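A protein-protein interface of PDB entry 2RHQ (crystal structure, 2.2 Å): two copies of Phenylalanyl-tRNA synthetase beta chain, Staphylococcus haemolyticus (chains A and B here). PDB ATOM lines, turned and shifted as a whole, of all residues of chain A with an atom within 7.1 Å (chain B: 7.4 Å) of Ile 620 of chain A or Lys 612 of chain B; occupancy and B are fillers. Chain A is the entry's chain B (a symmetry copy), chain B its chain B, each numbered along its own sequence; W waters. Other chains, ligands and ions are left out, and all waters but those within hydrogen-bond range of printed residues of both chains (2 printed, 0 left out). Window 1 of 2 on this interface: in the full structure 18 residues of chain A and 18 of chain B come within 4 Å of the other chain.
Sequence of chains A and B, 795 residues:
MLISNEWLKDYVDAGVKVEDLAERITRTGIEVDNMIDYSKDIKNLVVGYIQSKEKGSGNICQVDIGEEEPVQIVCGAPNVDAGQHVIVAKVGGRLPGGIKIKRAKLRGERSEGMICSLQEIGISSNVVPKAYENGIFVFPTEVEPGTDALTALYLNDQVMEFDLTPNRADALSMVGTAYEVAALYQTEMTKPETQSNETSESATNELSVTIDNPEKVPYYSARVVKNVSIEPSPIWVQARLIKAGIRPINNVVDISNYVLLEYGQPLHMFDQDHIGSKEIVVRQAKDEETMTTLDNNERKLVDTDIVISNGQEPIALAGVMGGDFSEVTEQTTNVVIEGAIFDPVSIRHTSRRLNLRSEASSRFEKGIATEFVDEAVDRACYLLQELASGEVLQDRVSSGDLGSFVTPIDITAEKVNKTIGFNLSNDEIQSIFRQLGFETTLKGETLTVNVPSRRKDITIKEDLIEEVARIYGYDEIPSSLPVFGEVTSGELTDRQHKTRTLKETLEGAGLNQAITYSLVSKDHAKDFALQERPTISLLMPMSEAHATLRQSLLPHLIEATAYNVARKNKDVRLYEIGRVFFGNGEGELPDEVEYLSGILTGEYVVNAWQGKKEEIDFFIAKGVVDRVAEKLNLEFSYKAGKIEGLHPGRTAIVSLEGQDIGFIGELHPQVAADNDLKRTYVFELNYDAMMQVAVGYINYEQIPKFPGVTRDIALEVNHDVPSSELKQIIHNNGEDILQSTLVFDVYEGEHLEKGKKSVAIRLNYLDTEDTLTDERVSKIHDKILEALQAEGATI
Water W2 bridges O of Glu 615 of chain A (2.5 Å) and NZ of Lys 612 of chain B (3.1 Å).
Water W1 lies within hydrogen-bond range of NZ of Lys 612 of chain B (2.6 Å), OE1 of Gln 610 of chain B (2.8 Å) and OD1 of Asp 617 of chain A (3.0 Å).
Positions printed for both chains: 603, 605 and 614.
The side-chain amide oxygen of Gln 610 of chain B lies within hydrogen-bond range of the side-chain amide nitrogen of Asn 607 of chain B.
The side-chain carboxylate of Asp 617 of chain A sits at hydrogen-bond distance from the backbone NH of Ile 620 of chain A, at 3.0 Å.
The backbone carbonyl oxygen of Glu 614 of chain A sits at hydrogen-bond distance from the backbone NH of Tyr 604 of chain A.
O of Val 605 of chain A lies within hydrogen-bond range of N of Glu 614 of chain A (2.6 Å).
The backbone NH (N) of Asn 607 of chain B is in hydrogen-bond range of the backbone carbonyl oxygen (O) of Lys 612 of chain B.
The side-chain carboxylate (OD1) of Asp 617 of chain A lies within hydrogen-bond range of the backbone NH (N) of Phe 619 of chain A (3.0 Å).
Printed residues of chain B that touch a printed residue of chain A: Trp 609, Gln 610 and Lys 612.
Hydrophobic or aromatic side chains of chain B that line the printed part of chain A: Trp 609.
Printed residues of chain B within 4 Å of Asp 617 of chain A: Gln 610 (3.2 Å).
Printed residues of chain B within 4 Å of Phe 619 of chain A: Trp 609 and Gln 610.
Ile 620 of chain A touches just one residue of chain B: Lys 612 (3.7 Å).
The nearest residue of chain A that does not touch Lys 612 of chain B is Asp 617 of chain A (4.6 Å).
NZ of Lys 612 of chain B lies within salt-bridge range of OE2 of Glu 614 of chain A (2.6 Å).
NE2 of Gln 610 of chain B sits at hydrogen-bond distance from OD2 of Asp 617 of chain A.
Among the printed residues, pairs that only touch across the chains: Phe 619 of chain A with Trp 609 of chain B (3.4 Å), Ile 620 of chain A with Lys 612 of chain B (3.7 Å) and Phe 619 of chain A with Gln 610 of chain B (3.8 Å).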
ATOM      1  N   LEU A 600     -23.619 -12.066 -13.285  1.00  0.00           N
ATOM      2  CA  LEU A 600     -24.904 -11.748 -13.894  1.00  0.00           C
ATOM      3  C   LEU A 600     -25.620 -13.017 -14.365  1.00  0.00           C
ATOM      4  O   LEU A 600     -25.056 -13.841 -15.033  1.00  0.00           O
ATOM      5  CB  LEU A 600     -24.712 -10.828 -15.143  1.00  0.00           C
ATOM      6  CG  LEU A 600     -23.843  -9.568 -15.002  1.00  0.00           C
ATOM      7  CD1 LEU A 600     -23.285  -9.092 -16.306  1.00  0.00           C
ATOM      8  CD2 LEU A 600     -24.558  -8.424 -14.243  1.00  0.00           C
ATOM      9  N   GLY A 602     -29.935 -14.326 -15.404  1.00  0.00           N
ATOM     10  CA  GLY A 602     -31.331 -13.974 -15.471  1.00  0.00           C
ATOM     11  C   GLY A 602     -31.672 -13.110 -16.675  1.00  0.00           C
ATOM     12  O   GLY A 602     -30.967 -13.151 -17.665  1.00  0.00           O
ATOM     13  N   GLU A 603     -32.768 -12.342 -16.560  1.00  0.00           N
ATOM     14  CA  GLU A 603     -33.191 -11.353 -17.555  1.00  0.00           C
ATOM     15  C   GLU A 603     -32.412 -10.034 -17.342  1.00  0.00           C
ATOM     16  O   GLU A 603     -32.099  -9.682 -16.216  1.00  0.00           O
ATOM     17  CB  GLU A 603     -34.708 -11.106 -17.411  1.00  0.00           C
ATOM     18  CG  GLU A 603     -35.607 -12.364 -17.469  1.00  0.00           C
ATOM     19  CD  GLU A 603     -36.920 -12.201 -16.650  1.00  0.00           C
ATOM     20  OE1 GLU A 603     -36.935 -11.360 -15.692  1.00  0.00           O
ATOM     21  OE2 GLU A 603     -37.925 -12.928 -16.953  1.00  0.00           O
ATOM     22  N   TYR A 604     -32.052  -9.324 -18.403  1.00  0.00           N
ATOM     23  CA  TYR A 604     -31.560  -7.958 -18.206  1.00  0.00           C
ATOM     24  C   TYR A 604     -32.691  -6.916 -18.265  1.00  0.00           C
ATOM     25  O   TYR A 604     -32.706  -5.958 -17.501  1.00  0.00           O
ATOM     26  CB  TYR A 604     -30.410  -7.600 -19.150  1.00  0.00           C
ATOM     27  CG  TYR A 604     -29.726  -6.315 -18.704  1.00  0.00           C
ATOM     28  CD1 TYR A 604     -29.609  -5.251 -19.548  1.00  0.00           C
ATOM     29  CD2 TYR A 604     -29.255  -6.165 -17.421  1.00  0.00           C
ATOM     30  CE1 TYR A 604     -29.011  -4.053 -19.147  1.00  0.00           C
ATOM     31  CE2 TYR A 604     -28.658  -4.953 -16.999  1.00  0.00           C
ATOM     32  CZ  TYR A 604     -28.558  -3.915 -17.885  1.00  0.00           C
ATOM     33  OH  TYR A 604     -27.990  -2.745 -17.536  1.00  0.00           O
ATOM     34  N   VAL A 605     -33.652  -7.181 -19.147  1.00  0.00           N
ATOM     35  CA  VAL A 605     -34.788  -6.331 -19.458  1.00  0.00           C
ATOM     36  C   VAL A 605     -35.978  -7.274 -19.565  1.00  0.00           C
ATOM     37  O   VAL A 605     -35.900  -8.291 -20.261  1.00  0.00           O
ATOM     38  CB  VAL A 605     -34.661  -5.713 -20.845  1.00  0.00           C
ATOM     39  CG1 VAL A 605     -35.988  -5.079 -21.287  1.00  0.00           C
ATOM     40  CG2 VAL A 605     -33.495  -4.754 -20.944  1.00  0.00           C
ATOM     41  N   GLU A 614     -35.255  -9.835 -22.315  1.00  0.00           N
ATOM     42  CA  GLU A 614     -33.920  -9.889 -22.868  1.00  0.00           C
ATOM     43  C   GLU A 614     -33.001 -10.656 -21.871  1.00  0.00           C
ATOM     44  O   GLU A 614     -32.699 -10.180 -20.782  1.00  0.00           O
ATOM     45  CB  GLU A 614     -33.437  -8.463 -23.241  1.00  0.00           C
ATOM     46  CG  GLU A 614     -31.963  -8.393 -23.631  1.00  0.00           C
ATOM     47  CD  GLU A 614     -31.416  -6.960 -23.819  1.00  0.00           C
ATOM     48  OE1 GLU A 614     -31.833  -5.979 -23.139  1.00  0.00           O
ATOM     49  OE2 GLU A 614     -30.504  -6.835 -24.650  1.00  0.00           O
ATOM     50  N   GLU A 615     -32.598 -11.869 -22.231  1.00  0.00           N
ATOM     51  CA  GLU A 615     -31.798 -12.685 -21.313  1.00  0.00           C
ATOM     52  C   GLU A 615     -30.342 -12.251 -21.314  1.00  0.00           C
ATOM     53  O   GLU A 615     -29.799 -11.872 -22.335  1.00  0.00           O
ATOM     54  CB  GLU A 615     -31.936 -14.179 -21.614  1.00  0.00           C
ATOM     55  CG  GLU A 615     -33.425 -14.681 -21.610  1.00  0.00           C
ATOM     56  CD  GLU A 615     -33.983 -15.063 -20.220  1.00  0.00           C
ATOM     57  OE1 GLU A 615     -34.121 -16.281 -19.968  1.00  0.00           O
ATOM     58  OE2 GLU A 615     -34.313 -14.168 -19.394  1.00  0.00           O
ATOM     59  N   ILE A 616     -29.726 -12.256 -20.141  1.00  0.00           N
ATOM     60  CA  ILE A 616     -28.349 -11.895 -20.048  1.00  0.00           C
ATOM     61  C   ILE A 616     -27.569 -12.863 -20.909  1.00  0.00           C
ATOM     62  O   ILE A 616     -27.732 -14.075 -20.811  1.00  0.00           O
ATOM     63  CB  ILE A 616     -27.876 -11.876 -18.615  1.00  0.00           C
ATOM     64  CG1 ILE A 616     -28.672 -10.817 -17.865  1.00  0.00           C
ATOM     65  CG2 ILE A 616     -26.373 -11.591 -18.522  1.00  0.00           C
ATOM     66  CD1 ILE A 616     -28.099 -10.412 -16.553  1.00  0.00           C
ATOM     67  N   ASP A 617     -26.727 -12.326 -21.774  1.00  0.00           N
ATOM     68  CA  ASP A 617     -25.743 -13.135 -22.396  1.00  0.00           C
ATOM     69  C   ASP A 617     -24.333 -12.569 -22.259  1.00  0.00           C
ATOM     70  O   ASP A 617     -24.067 -11.678 -21.458  1.00  0.00           O
ATOM     71  CB  ASP A 617     -26.143 -13.342 -23.855  1.00  0.00           C
ATOM     72  CG  ASP A 617     -25.888 -12.108 -24.696  1.00  0.00           C
ATOM     73  OD1 ASP A 617     -25.630 -11.024 -24.116  1.00  0.00           O
ATOM     74  OD2 ASP A 617     -25.923 -12.244 -25.916  1.00  0.00           O
ATOM     75  N   PHE A 618     -23.417 -13.099 -23.048  1.00  0.00           N
ATOM     76  CA  PHE A 618     -22.036 -12.681 -22.954  1.00  0.00           C
ATOM     77  C   PHE A 618     -21.883 -11.218 -23.355  1.00  0.00           C
ATOM     78  O   PHE A 618     -20.988 -10.490 -22.858  1.00  0.00           O
ATOM     79  CB  PHE A 618     -21.130 -13.617 -23.833  1.00  0.00           C
ATOM     80  CG  PHE A 618     -19.682 -13.189 -23.861  1.00  0.00           C
ATOM     81  CD1 PHE A 618     -19.248 -12.239 -24.774  1.00  0.00           C
ATOM     82  CD2 PHE A 618     -18.761 -13.707 -22.952  1.00  0.00           C
ATOM     83  CE1 PHE A 618     -17.933 -11.772 -24.761  1.00  0.00           C
ATOM     84  CE2 PHE A 618     -17.428 -13.251 -22.946  1.00  0.00           C
ATOM     85  CZ  PHE A 618     -17.019 -12.281 -23.836  1.00  0.00           C
ATOM     86  N   PHE A 619     -22.677 -10.765 -24.311  1.00  0.00           N
ATOM     87  CA  PHE A 619     -22.392  -9.434 -24.848  1.00  0.00           C
ATOM     88  C   PHE A 619     -22.958  -8.337 -23.953  1.00  0.00           C
ATOM     89  O   PHE A 619     -22.334  -7.249 -23.816  1.00  0.00           O
ATOM     90  CB  PHE A 619     -22.800  -9.350 -26.312  1.00  0.00           C
ATOM     91  CG  PHE A 619     -21.970 -10.230 -27.175  1.00  0.00           C
ATOM     92  CD1 PHE A 619     -22.473 -11.447 -27.617  1.00  0.00           C
ATOM     93  CD2 PHE A 619     -20.631  -9.888 -27.463  1.00  0.00           C
ATOM     94  CE1 PHE A 619     -21.689 -12.307 -28.371  1.00  0.00           C
ATOM     95  CE2 PHE A 619     -19.828 -10.742 -28.226  1.00  0.00           C
ATOM     96  CZ  PHE A 619     -20.362 -11.942 -28.690  1.00  0.00           C
ATOM     97  N   ILE A 620     -24.053  -8.673 -23.248  1.00  0.00           N
ATOM     98  CA  ILE A 620     -24.505  -7.887 -22.089  1.00  0.00           C
ATOM     99  C   ILE A 620     -23.441  -7.793 -21.059  1.00  0.00           C
ATOM    100  O   ILE A 620     -23.145  -6.731 -20.553  1.00  0.00           O
ATOM    101  CB  ILE A 620     -25.870  -8.381 -21.509  1.00  0.00           C
ATOM    102  CG1 ILE A 620     -26.954  -8.042 -22.507  1.00  0.00           C
ATOM    103  CG2 ILE A 620     -26.254  -7.653 -20.196  1.00  0.00           C
ATOM    104  CD1 ILE A 620     -28.212  -8.835 -22.310  1.00  0.00           C
ATOM    105  N   ALA A 621     -22.795  -8.904 -20.759  1.00  0.00           N
ATOM    106  CA  ALA A 621     -21.771  -8.838 -19.759  1.00  0.00           C
ATOM    107  C   ALA A 621     -20.593  -7.949 -20.219  1.00  0.00           C
ATOM    108  O   ALA A 621     -20.006  -7.204 -19.444  1.00  0.00           O
ATOM    109  CB  ALA A 621     -21.330 -10.220 -19.387  1.00  0.00           C
ATOM    110  N   LYS A 622     -20.225  -8.065 -21.475  1.00  0.00           N
ATOM    111  CA  LYS A 622     -19.219  -7.175 -22.076  1.00  0.00           C
ATOM    112  C   LYS A 622     -19.662  -5.692 -22.081  1.00  0.00           C
ATOM    113  O   LYS A 622     -18.861  -4.800 -21.882  1.00  0.00           O
ATOM    114  CB  LYS A 622     -19.007  -7.634 -23.526  1.00  0.00           C
ATOM    115  CG  LYS A 622     -17.670  -7.131 -24.151  1.00  0.00           C
ATOM    116  CD  LYS A 622     -17.592  -7.561 -25.586  1.00  0.00           C
ATOM    117  CE  LYS A 622     -16.431  -6.910 -26.375  1.00  0.00           C
ATOM    118  NZ  LYS A 622     -16.361  -7.500 -27.824  1.00  0.00           N
ATOM    119  N   GLY A 623     -20.950  -5.467 -22.351  1.00  0.00           N
ATOM    120  CA  GLY A 623     -21.551  -4.154 -22.314  1.00  0.00           C
ATOM    121  C   GLY A 623     -21.322  -3.540 -20.977  1.00  0.00           C
ATOM    122  O   GLY A 623     -20.977  -2.387 -20.877  1.00  0.00           O
ATOM    123  N   VAL A 624     -21.507  -4.317 -19.919  1.00  0.00           N
ATOM    124  CA  VAL A 624     -21.204  -3.792 -18.586  1.00  0.00           C
ATOM    125  C   VAL A 624     -19.753  -3.350 -18.550  1.00  0.00           C
ATOM    126  O   VAL A 624     -19.420  -2.256 -18.069  1.00  0.00           O
ATOM    127  CB  VAL A 624     -21.469  -4.855 -17.477  1.00  0.00           C
ATOM    128  CG1 VAL A 624     -21.076  -4.320 -16.126  1.00  0.00           C
ATOM    129  CG2 VAL A 624     -22.898  -5.264 -17.443  1.00  0.00           C
ATOM    130  N   VAL A 625     -18.855  -4.199 -19.060  1.00  0.00           N
ATOM    131  CA  VAL A 625     -17.431  -3.934 -18.916  1.00  0.00           C
ATOM    132  C   VAL A 625     -17.026  -2.777 -19.867  1.00  0.00           C
ATOM    133  O   VAL A 625     -16.237  -1.894 -19.485  1.00  0.00           O
ATOM    134  CB  VAL A 625     -16.581  -5.209 -19.200  1.00  0.00           C
ATOM    135  CG1 VAL A 625     -15.046  -4.906 -19.112  1.00  0.00           C
ATOM    136  CG2 VAL A 625     -16.992  -6.334 -18.231  1.00  0.00           C
ATOM    137  N   ASP A 626     -17.566  -2.778 -21.085  1.00  0.00           N
ATOM    138  CA  ASP A 626     -17.462  -1.583 -21.962  1.00  0.00           C
ATOM    139  C   ASP A 626     -17.915  -0.316 -21.272  1.00  0.00           C
ATOM    140  O   ASP A 626     -17.303   0.727 -21.408  1.00  0.00           O
ATOM    141  CB  ASP A 626     -18.272  -1.759 -23.236  1.00  0.00           C
ATOM    142  CG  ASP A 626     -17.500  -2.517 -24.330  1.00  0.00           C
ATOM    143  OD1 ASP A 626     -18.112  -3.112 -25.250  1.00  0.00           O
ATOM    144  OD2 ASP A 626     -16.273  -2.523 -24.228  1.00  0.00           O
ATOM    145  N   ILE A 664     -13.755 -11.835 -18.890  1.00  0.00           N
ATOM    146  CA  ILE A 664     -15.197 -11.950 -18.798  1.00  0.00           C
ATOM    147  C   ILE A 664     -15.393 -13.331 -19.302  1.00  0.00           C
ATOM    148  O   ILE A 664     -14.656 -13.738 -20.173  1.00  0.00           O
ATOM    149  CB  ILE A 664     -15.948 -11.001 -19.813  1.00  0.00           C
ATOM    150  CG1 ILE A 664     -15.674  -9.572 -19.512  1.00  0.00           C
ATOM    151  CG2 ILE A 664     -17.496 -11.238 -19.811  1.00  0.00           C
ATOM    152  CD1 ILE A 664     -15.689  -8.743 -20.807  1.00  0.00           C
ATOM    153  N   TYR A 681     -22.663 -15.231 -16.191  1.00  0.00           N
ATOM    154  CA  TYR A 681     -21.449 -14.532 -16.660  1.00  0.00           C
ATOM    155  C   TYR A 681     -20.800 -13.825 -15.511  1.00  0.00           C
ATOM    156  O   TYR A 681     -21.497 -13.307 -14.628  1.00  0.00           O
ATOM    157  CB  TYR A 681     -21.862 -13.509 -17.763  1.00  0.00           C
ATOM    158  CG  TYR A 681     -22.635 -14.259 -18.834  1.00  0.00           C
ATOM    159  CD1 TYR A 681     -21.981 -14.780 -19.944  1.00  0.00           C
ATOM    160  CD2 TYR A 681     -23.969 -14.541 -18.677  1.00  0.00           C
ATOM    161  CE1 TYR A 681     -22.651 -15.541 -20.882  1.00  0.00           C
ATOM    162  CE2 TYR A 681     -24.655 -15.283 -19.623  1.00  0.00           C
ATOM    163  CZ  TYR A 681     -23.969 -15.801 -20.712  1.00  0.00           C
ATOM    164  OH  TYR A 681     -24.643 -16.564 -21.632  1.00  0.00           O
ATOM    165  N   GLU B 603     -33.800   4.400 -31.039  1.00  0.00           N
ATOM    166  CA  GLU B 603     -33.596   3.107 -30.379  1.00  0.00           C
ATOM    167  C   GLU B 603     -33.261   3.333 -28.886  1.00  0.00           C
ATOM    168  O   GLU B 603     -32.615   4.311 -28.544  1.00  0.00           O
ATOM    169  CB  GLU B 603     -32.440   2.359 -31.077  1.00  0.00           C
ATOM    170  CG  GLU B 603     -32.578   2.179 -32.608  1.00  0.00           C
ATOM    171  CD  GLU B 603     -31.201   2.105 -33.330  1.00  0.00           C
ATOM    172  OE1 GLU B 603     -30.192   2.642 -32.765  1.00  0.00           O
ATOM    173  OE2 GLU B 603     -31.136   1.529 -34.467  1.00  0.00           O
ATOM    174  N   VAL B 605     -32.040   0.454 -27.110  1.00  0.00           N
ATOM    175  CA  VAL B 605     -31.068  -0.624 -27.050  1.00  0.00           C
ATOM    176  C   VAL B 605     -30.888  -1.082 -28.491  1.00  0.00           C
ATOM    177  O   VAL B 605     -31.877  -1.327 -29.190  1.00  0.00           O
ATOM    178  CB  VAL B 605     -31.628  -1.842 -26.328  1.00  0.00           C
ATOM    179  CG1 VAL B 605     -30.729  -3.068 -26.539  1.00  0.00           C
ATOM    180  CG2 VAL B 605     -31.905  -1.568 -24.865  1.00  0.00           C
ATOM    181  N   VAL B 606     -29.635  -1.197 -28.914  1.00  0.00           N
ATOM    182  CA  VAL B 606     -29.295  -1.610 -30.255  1.00  0.00           C
ATOM    183  C   VAL B 606     -28.010  -2.451 -30.192  1.00  0.00           C
ATOM    184  O   VAL B 606     -27.047  -2.091 -29.516  1.00  0.00           O
ATOM    185  CB  VAL B 606     -29.127  -0.375 -31.187  1.00  0.00           C
ATOM    186  CG1 VAL B 606     -27.996   0.519 -30.715  1.00  0.00           C
ATOM    187  CG2 VAL B 606     -28.904  -0.794 -32.635  1.00  0.00           C
ATOM    188  N   ASN B 607     -28.038  -3.604 -30.853  1.00  0.00           N
ATOM    189  CA  ASN B 607     -26.813  -4.326 -31.244  1.00  0.00           C
ATOM    190  C   ASN B 607     -27.113  -4.981 -32.561  1.00  0.00           C
ATOM    191  O   ASN B 607     -27.691  -6.065 -32.601  1.00  0.00           O
ATOM    192  CB  ASN B 607     -26.424  -5.407 -30.185  1.00  0.00           C
ATOM    193  CG  ASN B 607     -24.917  -5.651 -30.123  1.00  0.00           C
ATOM    194  OD1 ASN B 607     -24.149  -4.888 -30.696  1.00  0.00           O
ATOM    195  ND2 ASN B 607     -24.492  -6.714 -29.424  1.00  0.00           N
ATOM    196  N   ALA B 608     -26.754  -4.323 -33.658  1.00  0.00           N
ATOM    197  CA  ALA B 608     -27.279  -4.708 -34.975  1.00  0.00           C
ATOM    198  C   ALA B 608     -26.907  -6.152 -35.318  1.00  0.00           C
ATOM    199  O   ALA B 608     -27.749  -6.930 -35.778  1.00  0.00           O
ATOM    200  CB  ALA B 608     -26.745  -3.755 -36.055  1.00  0.00           C
ATOM    201  N   TRP B 609     -25.635  -6.491 -35.123  1.00  0.00           N
ATOM    202  CA  TRP B 609     -25.142  -7.786 -35.539  1.00  0.00           C
ATOM    203  C   TRP B 609     -25.906  -8.916 -34.849  1.00  0.00           C
ATOM    204  O   TRP B 609     -26.065  -9.971 -35.428  1.00  0.00           O
ATOM    205  CB  TRP B 609     -23.619  -7.905 -35.316  1.00  0.00           C
ATOM    206  CG  TRP B 609     -23.177  -8.313 -33.928  1.00  0.00           C
ATOM    207  CD1 TRP B 609     -22.633  -7.509 -32.978  1.00  0.00           C
ATOM    208  CD2 TRP B 609     -23.190  -9.640 -33.368  1.00  0.00           C
ATOM    209  NE1 TRP B 609     -22.333  -8.234 -31.845  1.00  0.00           N
ATOM    210  CE2 TRP B 609     -22.653  -9.549 -32.066  1.00  0.00           C
ATOM    211  CE3 TRP B 609     -23.596 -10.901 -33.846  1.00  0.00           C
ATOM    212  CZ2 TRP B 609     -22.531 -10.671 -31.219  1.00  0.00           C
ATOM    213  CZ3 TRP B 609     -23.478 -12.017 -32.999  1.00  0.00           C
ATOM    214  CH2 TRP B 609     -22.969 -11.884 -31.700  1.00  0.00           C
ATOM    215  N   GLN B 610     -26.419  -8.687 -33.635  1.00  0.00           N
ATOM    216  CA  GLN B 610     -27.286  -9.688 -33.007  1.00  0.00           C
ATOM    217  C   GLN B 610     -28.750  -9.600 -33.432  1.00  0.00           C
ATOM    218  O   GLN B 610     -29.551 -10.426 -33.036  1.00  0.00           O
ATOM    219  CB  GLN B 610     -27.218  -9.590 -31.498  1.00  0.00           C
ATOM    220  CG  GLN B 610     -25.906  -9.903 -30.942  1.00  0.00           C
ATOM    221  CD  GLN B 610     -25.945  -9.981 -29.444  1.00  0.00           C
ATOM    222  OE1 GLN B 610     -25.699  -8.993 -28.724  1.00  0.00           O
ATOM    223  NE2 GLN B 610     -26.269 -11.161 -28.954  1.00  0.00           N
ATOM    224  N   GLY B 611     -29.111  -8.601 -34.228  1.00  0.00           N
ATOM    225  CA  GLY B 611     -30.528  -8.341 -34.522  1.00  0.00           C
ATOM    226  C   GLY B 611     -31.257  -7.738 -33.343  1.00  0.00           C
ATOM    227  O   GLY B 611     -32.452  -7.833 -33.251  1.00  0.00           O
ATOM    228  N   LYS B 612     -30.542  -7.085 -32.443  1.00  0.00           N
ATOM    229  CA  LYS B 612     -31.212  -6.395 -31.352  1.00  0.00           C
ATOM    230  C   LYS B 612     -31.528  -4.963 -31.728  1.00  0.00           C
ATOM    231  O   LYS B 612     -30.638  -4.185 -32.049  1.00  0.00           O
ATOM    232  CB  LYS B 612     -30.345  -6.408 -30.082  1.00  0.00           C
ATOM    233  CG  LYS B 612     -30.244  -7.786 -29.400  1.00  0.00           C
ATOM    234  CD  LYS B 612     -29.862  -7.642 -27.906  1.00  0.00           C
ATOM    235  CE  LYS B 612     -29.853  -8.992 -27.178  1.00  0.00           C
ATOM    236  NZ  LYS B 612     -29.317  -8.835 -25.822  1.00  0.00           N
ATOM    237  N   LYS B 613     -32.806  -4.612 -31.656  1.00  0.00           N
ATOM    238  CA  LYS B 613     -33.209  -3.226 -31.793  1.00  0.00           C
ATOM    239  C   LYS B 613     -34.433  -2.961 -30.918  1.00  0.00           C
ATOM    240  O   LYS B 613     -35.506  -3.448 -31.181  1.00  0.00           O
ATOM    241  CB  LYS B 613     -33.484  -2.899 -33.278  1.00  0.00           C
ATOM    242  CG  LYS B 613     -33.704  -1.409 -33.523  1.00  0.00           C
ATOM    243  CD  LYS B 613     -33.460  -0.973 -34.995  1.00  0.00           C
ATOM    244  CE  LYS B 613     -34.195  -1.838 -35.997  1.00  0.00           C
ATOM    245  NZ  LYS B 613     -34.382  -1.113 -37.310  1.00  0.00           N
ATOM    246  N   GLU B 614     -34.283  -2.226 -29.836  1.00  0.00           N
ATOM    247  CA  GLU B 614     -35.462  -1.955 -29.043  1.00  0.00           C
ATOM    248  C   GLU B 614     -35.856  -0.460 -29.235  1.00  0.00           C
ATOM    249  O   GLU B 614     -35.159   0.448 -28.795  1.00  0.00           O
ATOM    250  CB  GLU B 614     -35.228  -2.387 -27.571  1.00  0.00           C
ATOM    251  CG  GLU B 614     -36.333  -1.945 -26.616  1.00  0.00           C
ATOM    252  CD  GLU B 614     -36.027  -2.196 -25.122  1.00  0.00           C
ATOM    253  OE1 GLU B 614     -34.857  -2.132 -24.648  1.00  0.00           O
ATOM    254  OE2 GLU B 614     -37.011  -2.419 -24.400  1.00  0.00           O
HETATM  255  O   HOH W   1     -26.768  -9.066 -26.091  1.00  0.00           O
HETATM  256  O   HOH W   2     -30.219 -11.586 -24.810  1.00  0.00           O
